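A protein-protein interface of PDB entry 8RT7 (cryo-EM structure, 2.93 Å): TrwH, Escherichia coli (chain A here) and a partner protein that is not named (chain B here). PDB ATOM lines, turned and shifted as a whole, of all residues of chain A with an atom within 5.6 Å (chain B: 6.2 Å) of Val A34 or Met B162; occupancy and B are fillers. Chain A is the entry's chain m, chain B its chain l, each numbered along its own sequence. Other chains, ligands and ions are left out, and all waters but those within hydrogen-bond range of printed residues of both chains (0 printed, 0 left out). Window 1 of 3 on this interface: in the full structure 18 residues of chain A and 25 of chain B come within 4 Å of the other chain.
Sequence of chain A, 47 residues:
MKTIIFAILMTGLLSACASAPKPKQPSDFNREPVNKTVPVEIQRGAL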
ATOM      1  N   ASN A  30       2.617 -17.179 -21.877  1.00  0.00           N
ATOM      2  CA  ASN A  30       2.030 -15.852 -22.027  1.00  0.00           C
ATOM      3  C   ASN A  30       3.107 -14.806 -22.315  1.00  0.00           C
ATOM      4  O   ASN A  30       3.351 -13.889 -21.532  1.00  0.00           O
ATOM      5  CB  ASN A  30       1.245 -15.498 -20.773  1.00  0.00           C
ATOM      6  CG  ASN A  30       2.041 -15.744 -19.502  1.00  0.00           C
ATOM      7  OD1 ASN A  30       3.189 -16.176 -19.553  1.00  0.00           O
ATOM      8  ND2 ASN A  30       1.437 -15.453 -18.358  1.00  0.00           N
ATOM      9  N   ARG A  31       3.758 -14.953 -23.466  1.00  0.00           N
ATOM     10  CA  ARG A  31       4.864 -14.080 -23.835  1.00  0.00           C
ATOM     11  C   ARG A  31       4.334 -12.903 -24.639  1.00  0.00           C
ATOM     12  O   ARG A  31       3.683 -13.091 -25.670  1.00  0.00           O
ATOM     13  CB  ARG A  31       5.927 -14.838 -24.625  1.00  0.00           C
ATOM     14  CG  ARG A  31       7.191 -14.033 -24.797  1.00  0.00           C
ATOM     15  CD  ARG A  31       8.101 -14.604 -25.856  1.00  0.00           C
ATOM     16  NE  ARG A  31       8.909 -15.699 -25.344  1.00  0.00           N
ATOM     17  CZ  ARG A  31      10.230 -15.752 -25.441  1.00  0.00           C
ATOM     18  NH1 ARG A  31      10.894 -14.770 -26.030  1.00  0.00           N
ATOM     19  NH2 ARG A  31      10.887 -16.790 -24.947  1.00  0.00           N
ATOM     20  N   GLU A  32       4.619 -11.695 -24.173  1.00  0.00           N
ATOM     21  CA  GLU A  32       4.034 -10.493 -24.742  1.00  0.00           C
ATOM     22  C   GLU A  32       5.021  -9.354 -24.574  1.00  0.00           C
ATOM     23  O   GLU A  32       5.886  -9.403 -23.694  1.00  0.00           O
ATOM     24  CB  GLU A  32       2.704 -10.152 -24.064  1.00  0.00           C
ATOM     25  CG  GLU A  32       2.838  -9.778 -22.611  1.00  0.00           C
ATOM     26  CD  GLU A  32       1.504  -9.515 -21.960  1.00  0.00           C
ATOM     27  OE1 GLU A  32       0.474  -9.654 -22.646  1.00  0.00           O
ATOM     28  OE2 GLU A  32       1.479  -9.154 -20.769  1.00  0.00           O
ATOM     29  N   PRO A  33       4.929  -8.321 -25.408  1.00  0.00           N
ATOM     30  CA  PRO A  33       5.833  -7.177 -25.265  1.00  0.00           C
ATOM     31  C   PRO A  33       5.708  -6.514 -23.903  1.00  0.00           C
ATOM     32  O   PRO A  33       4.615  -6.382 -23.353  1.00  0.00           O
ATOM     33  CB  PRO A  33       5.381  -6.238 -26.385  1.00  0.00           C
ATOM     34  CG  PRO A  33       4.770  -7.124 -27.381  1.00  0.00           C
ATOM     35  CD  PRO A  33       4.122  -8.231 -26.633  1.00  0.00           C
ATOM     36  N   VAL A  34       6.849  -6.099 -23.356  1.00  0.00           N
ATOM     37  CA  VAL A  34       6.829  -5.271 -22.157  1.00  0.00           C
ATOM     38  C   VAL A  34       6.305  -3.883 -22.487  1.00  0.00           C
ATOM     39  O   VAL A  34       5.478  -3.325 -21.761  1.00  0.00           O
ATOM     40  CB  VAL A  34       8.229  -5.198 -21.525  1.00  0.00           C
ATOM     41  CG1 VAL A  34       8.197  -4.339 -20.302  1.00  0.00           C
ATOM     42  CG2 VAL A  34       8.725  -6.563 -21.174  1.00  0.00           C
ATOM     43  N   ASN A  35       6.770  -3.311 -23.591  1.00  0.00           N
ATOM     44  CA  ASN A  35       6.520  -1.913 -23.913  1.00  0.00           C
ATOM     45  C   ASN A  35       5.221  -1.813 -24.694  1.00  0.00           C
ATOM     46  O   ASN A  35       5.193  -2.029 -25.906  1.00  0.00           O
ATOM     47  CB  ASN A  35       7.683  -1.331 -24.703  1.00  0.00           C
ATOM     48  CG  ASN A  35       8.940  -1.230 -23.886  1.00  0.00           C
ATOM     49  OD1 ASN A  35       9.145  -0.257 -23.174  1.00  0.00           O
ATOM     50  ND2 ASN A  35       9.791  -2.235 -23.980  1.00  0.00           N
ATOM     51  N   LYS A  36       4.138  -1.483 -23.999  1.00  0.00           N
ATOM     52  CA  LYS A  36       2.907  -1.146 -24.698  1.00  0.00           C
ATOM     53  C   LYS A  36       2.996   0.231 -25.333  1.00  0.00           C
ATOM     54  O   LYS A  36       2.412   0.461 -26.395  1.00  0.00           O
ATOM     55  CB  LYS A  36       1.720  -1.220 -23.743  1.00  0.00           C
ATOM     56  CG  LYS A  36       1.040  -2.569 -23.718  1.00  0.00           C
ATOM     57  CD  LYS A  36       1.804  -3.561 -22.870  1.00  0.00           C
ATOM     58  CE  LYS A  36       1.063  -4.875 -22.781  1.00  0.00           C
ATOM     59  NZ  LYS A  36       1.806  -5.891 -22.006  1.00  0.00           N
ATOM     60  N   TYR B 160      11.792  -5.882 -26.107  1.00  0.00           N
ATOM     61  CA  TYR B 160      11.779  -6.619 -24.855  1.00  0.00           C
ATOM     62  C   TYR B 160      10.439  -7.311 -24.696  1.00  0.00           C
ATOM     63  O   TYR B 160       9.395  -6.709 -24.955  1.00  0.00           O
ATOM     64  CB  TYR B 160      12.040  -5.688 -23.676  1.00  0.00           C
ATOM     65  CG  TYR B 160      13.500  -5.481 -23.401  1.00  0.00           C
ATOM     66  CD1 TYR B 160      14.225  -4.526 -24.083  1.00  0.00           C
ATOM     67  CD2 TYR B 160      14.156  -6.250 -22.466  1.00  0.00           C
ATOM     68  CE1 TYR B 160      15.551  -4.344 -23.842  1.00  0.00           C
ATOM     69  CE2 TYR B 160      15.483  -6.074 -22.219  1.00  0.00           C
ATOM     70  CZ  TYR B 160      16.175  -5.121 -22.907  1.00  0.00           C
ATOM     71  OH  TYR B 160      17.510  -4.952 -22.650  1.00  0.00           O
ATOM     72  N   MET B 161      10.469  -8.569 -24.281  1.00  0.00           N
ATOM     73  CA  MET B 161       9.258  -9.339 -24.049  1.00  0.00           C
ATOM     74  C   MET B 161       9.286  -9.973 -22.668  1.00  0.00           C
ATOM     75  O   MET B 161      10.316 -10.021 -21.998  1.00  0.00           O
ATOM     76  CB  MET B 161       9.074 -10.398 -25.135  1.00  0.00           C
ATOM     77  CG  MET B 161       8.964  -9.795 -26.508  1.00  0.00           C
ATOM     78  SD  MET B 161       7.773 -10.647 -27.543  1.00  0.00           S
ATOM     79  CE  MET B 161       7.840  -9.620 -29.006  1.00  0.00           C
ATOM     80  N   MET B 162       8.123 -10.447 -22.236  1.00  0.00           N
ATOM     81  CA  MET B 162       7.972 -10.943 -20.880  1.00  0.00           C
ATOM     82  C   MET B 162       6.974 -12.084 -20.859  1.00  0.00           C
ATOM     83  O   MET B 162       6.019 -12.097 -21.635  1.00  0.00           O
ATOM     84  CB  MET B 162       7.525  -9.829 -19.929  1.00  0.00           C
ATOM     85  CG  MET B 162       6.056  -9.492 -19.979  1.00  0.00           C
ATOM     86  SD  MET B 162       5.712  -7.903 -19.234  1.00  0.00           S
ATOM     87  CE  MET B 162       4.159  -7.505 -20.009  1.00  0.00           C
ATOM     88  N   SER B 163       7.207 -13.044 -19.970  1.00  0.00           N
ATOM     89  CA  SER B 163       6.323 -14.189 -19.823  1.00  0.00           C
ATOM     90  C   SER B 163       6.455 -14.734 -18.412  1.00  0.00           C
ATOM     91  O   SER B 163       7.547 -15.124 -17.997  1.00  0.00           O
ATOM     92  CB  SER B 163       6.656 -15.274 -20.845  1.00  0.00           C
ATOM     93  OG  SER B 163       8.002 -15.681 -20.721  1.00  0.00           O
ATOM     94  N   GLY B 164       5.348 -14.759 -17.681  1.00  0.00           N
ATOM     95  CA  GLY B 164       5.362 -15.250 -16.322  1.00  0.00           C
ATOM     96  C   GLY B 164       4.275 -14.630 -15.477  1.00  0.00           C
ATOM     97  O   GLY B 164       3.112 -14.599 -15.881  1.00  0.00           O
ATOM     98  N   LYS B 166       2.642 -11.596 -14.526  1.00  0.00           N
ATOM     99  CA  LYS B 166       2.558 -10.228 -15.013  1.00  0.00           C
ATOM    100  C   LYS B 166       2.175  -9.232 -13.935  1.00  0.00           C
ATOM    101  O   LYS B 166       2.202  -8.028 -14.199  1.00  0.00           O
ATOM    102  CB  LYS B 166       1.553 -10.123 -16.154  1.00  0.00           C
ATOM    103  CG  LYS B 166       1.736 -11.137 -17.246  1.00  0.00           C
ATOM    104  CD  LYS B 166       3.096 -11.038 -17.867  1.00  0.00           C
ATOM    105  CE  LYS B 166       3.037 -11.486 -19.301  1.00  0.00           C
ATOM    106  NZ  LYS B 166       2.231 -12.709 -19.435  1.00  0.00           N
ATOM    107  N   ALA B 169       5.179  -7.098 -13.355  1.00  0.00           N
ATOM    108  CA  ALA B 169       5.886  -6.714 -14.560  1.00  0.00           C
ATOM    109  C   ALA B 169       6.170  -5.216 -14.577  1.00  0.00           C
ATOM    110  O   ALA B 169       5.459  -4.435 -13.944  1.00  0.00           O
ATOM    111  CB  ALA B 169       5.071  -7.093 -15.787  1.00  0.00           C
ATOM    112  N   PRO B 170       7.212  -4.790 -15.284  1.00  0.00           N
ATOM    113  CA  PRO B 170       7.415  -3.362 -15.508  1.00  0.00           C
ATOM    114  C   PRO B 170       6.376  -2.827 -16.474  1.00  0.00           C
ATOM    115  O   PRO B 170       5.706  -3.575 -17.186  1.00  0.00           O
ATOM    116  CB  PRO B 170       8.811  -3.298 -16.134  1.00  0.00           C
ATOM    117  CG  PRO B 170       9.448  -4.546 -15.773  1.00  0.00           C
ATOM    118  CD  PRO B 170       8.372  -5.566 -15.738  1.00  0.00           C
ATOM    119  N   VAL B 171       6.246  -1.503 -16.497  1.00  0.00           N
ATOM    120  CA  VAL B 171       5.432  -0.905 -17.545  1.00  0.00           C
ATOM    121  C   VAL B 171       6.249  -0.643 -18.797  1.00  0.00           C
ATOM    122  O   VAL B 171       5.672  -0.491 -19.879  1.00  0.00           O
ATOM    123  CB  VAL B 171       4.756   0.393 -17.075  1.00  0.00           C
ATOM    124  CG1 VAL B 171       3.676   0.087 -16.078  1.00  0.00           C
ATOM    125  CG2 VAL B 171       5.755   1.326 -16.470  1.00  0.00           C
ATOM    126  N   ASN B 172       7.575  -0.601 -18.686  1.00  0.00           N
ATOM    127  CA  ASN B 172       8.450  -0.338 -19.819  1.00  0.00           C
ATOM    128  C   ASN B 172       9.838  -0.862 -19.498  1.00  0.00           C
ATOM    129  O   ASN B 172      10.309  -0.720 -18.372  1.00  0.00           O
ATOM    130  CB  ASN B 172       8.516   1.157 -20.135  1.00  0.00           C
ATOM    131  CG  ASN B 172       7.421   1.596 -21.065  1.00  0.00           C
ATOM    132  OD1 ASN B 172       6.683   2.531 -20.774  1.00  0.00           O
ATOM    133  ND2 ASN B 172       7.298   0.914 -22.189  1.00  0.00           N
ATOM    134  N   ALA B 173      10.487  -1.454 -20.494  1.00  0.00           N
ATOM    135  CA  ALA B 173      11.861  -1.912 -20.366  1.00  0.00           C
ATOM    136  C   ALA B 173      12.617  -1.591 -21.646  1.00  0.00           C
ATOM    137  O   ALA B 173      12.081  -1.737 -22.744  1.00  0.00           O
ATOM    138  CB  ALA B 173      11.933  -3.410 -20.072  1.00  0.00           C
ATOM    139  N   LEU B 235       8.859 -13.411 -13.048  1.00  0.00           N
ATOM    140  CA  LEU B 235       8.625 -12.941 -14.402  1.00  0.00           C
ATOM    141  C   LEU B 235       9.942 -12.972 -15.155  1.00  0.00           C
ATOM    142  O   LEU B 235      10.938 -12.428 -14.679  1.00  0.00           O
ATOM    143  CB  LEU B 235       8.060 -11.527 -14.395  1.00  0.00           C
ATOM    144  CG  LEU B 235       7.768 -10.883 -15.740  1.00  0.00           C
ATOM    145  CD1 LEU B 235       6.410 -11.262 -16.241  1.00  0.00           C
ATOM    146  CD2 LEU B 235       7.893  -9.411 -15.604  1.00  0.00           C
ATOM    147  N   ALA B 236       9.944 -13.590 -16.329  1.00  0.00           N
ATOM    148  CA  ALA B 236      11.129 -13.650 -17.173  1.00  0.00           C
ATOM    149  C   ALA B 236      11.040 -12.586 -18.253  1.00  0.00           C
ATOM    150  O   ALA B 236       9.996 -12.433 -18.889  1.00  0.00           O
ATOM    151  CB  ALA B 236      11.282 -15.028 -17.806  1.00  0.00           C
ATOM    152  N   ILE B 237      12.129 -11.853 -18.449  1.00  0.00           N
ATOM    153  CA  ILE B 237      12.225 -10.809 -19.459  1.00  0.00           C
ATOM    154  C   ILE B 237      13.191 -11.283 -20.531  1.00  0.00           C
ATOM    155  O   ILE B 237      14.202 -11.919 -20.225  1.00  0.00           O
ATOM    156  CB  ILE B 237      12.697  -9.474 -18.856  1.00  0.00           C
ATOM    157  CG1 ILE B 237      11.813  -9.059 -17.684  1.00  0.00           C
ATOM    158  CG2 ILE B 237      12.665  -8.385 -19.899  1.00  0.00           C
ATOM    159  CD1 ILE B 237      10.465  -8.568 -18.079  1.00  0.00           C
ATOM    160  N   PHE B 238      12.875 -10.985 -21.788  1.00  0.00           N
ATOM    161  CA  PHE B 238      13.683 -11.416 -22.918  1.00  0.00           C
ATOM    162  C   PHE B 238      14.075 -10.221 -23.765  1.00  0.00           C
ATOM    163  O   PHE B 238      13.216  -9.443 -24.180  1.00  0.00           O
ATOM    164  CB  PHE B 238      12.934 -12.433 -23.770  1.00  0.00           C
ATOM    165  CG  PHE B 238      12.496 -13.642 -23.011  1.00  0.00           C
ATOM    166  CD1 PHE B 238      13.354 -14.698 -22.817  1.00  0.00           C
ATOM    167  CD2 PHE B 238      11.227 -13.717 -22.484  1.00  0.00           C
ATOM    168  CE1 PHE B 238      12.953 -15.800 -22.124  1.00  0.00           C
ATOM    169  CE2 PHE B 238      10.826 -14.824 -21.788  1.00  0.00           C
ATOM    170  CZ  PHE B 238      11.690 -15.862 -21.605  1.00  0.00           C
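The backbone carbonyl oxygen of Tyr B160 sits at hydrogen-bond distance from the backbone NH of Val A34, 3.1 Å away. N of Met B162 is in hydrogen-bond range of O of Glu A32 (2.9 Å). The side-chain amide nitrogen of Asn A30 lies within hydrogen-bond range of the backbone carbonyl oxygen of Gly B164 (3.1 Å). The side-chain amino group (NZ) of Lys B166 sits at hydrogen-bond distance from the backbone carbonyl oxygen (O) of Asn A30, at 2.7 Å. The side-chain amino group (NZ) of Lys B166 lies within salt-bridge range of the side-chain carboxylate (OE2) of Glu A32. The backbone carbonyl oxygen of Ala B173 sits at hydrogen-bond distance from the side-chain amide nitrogen of Asn A35 (2.6 Å). O of Met B162 sits close to O of Asn A30 (3.2 Å). The backbone carbonyl oxygen (O) of Val A34 lies close to the backbone carbonyl oxygen (O) of Val B171 (3.4 Å). The side-chain amide nitrogen of Asn B172 sits close to the side-chain amide oxygen of Asn A35 (2.4 Å).
The backbone NH of Phe B238 lies within hydrogen-bond range of the backbone carbonyl oxygen of Met B161 (2.7 Å). N of Ser B163 sits at hydrogen-bond distance from O of Ala B236 (3.1 Å). OE2 of Glu A32 is in salt-bridge range of NZ of Lys A36, 3.5 Å away. NZ of Lys A36 sits at hydrogen-bond distance from O of Pro A33 (3.2 Å).
Ser B163 touches Asn A30. Met B162 touches Arg A31 (O to CA, 3.2 Å). Arg A31 touches Ser B163 (CA to CB, 3.7 Å). Arg A31 touches Phe B238 (NH2 to CZ, 3.6 Å). Met B161 touches Glu A32. Pro A33 touches Met B162 (O to CE, 3.6 Å). Met B161 touches Val A34. CG2 of Val A34 touches CB of Met B162, at 3.7 Å. Val A34 touches Asn B172. Val A34 touches Ala B173.
Of chain B, only Tyr B160, Met B161, Met B162, Val B171, Asn B172 and Ala B173 come within 4 Å of Val A34. Printed residues of chain A within 4 Å of Met B162: Asn A30 (3.2 Å), Arg A31 (3.2 Å), Glu A32 (2.9 Å), Pro A33 (3.6 Å), Val A34 (3.7 Å) and Lys A36 (3.5 Å). Printed residues of chain A within 4 Å of Ser B163: Asn A30 (3.4 Å) and Arg A31 (3.7 Å). Printed residues of chain A within 4 Å of Gly B164: Asn A30. Printed residues of chain A within 4 Å of Val B171: Val A34 (3.4 Å). Ile B237 touches none of the printed residues of chain A. The nearest printed residue of chain A that does not touch Met B162 is Asn A35 (6.1 Å). The nearest printed residue of chain A that does not touch Tyr B160 is Asn A35 (4.1 Å).
Of the 7 printed residues of chain A, 7 touch a printed residue of chain B. Hydrophobic or aromatic side chains of chain B that line the printed part of chain A: Met B161, Met B162, Ala B173 and Phe B238. Among the printed residues, 21 pairs touch across the chains. Among the printed residues, Asp or Glu carboxylates within 4 Å of a Lys or Arg side-chain nitrogen of the other chain: Glu A32 with Lys B166.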
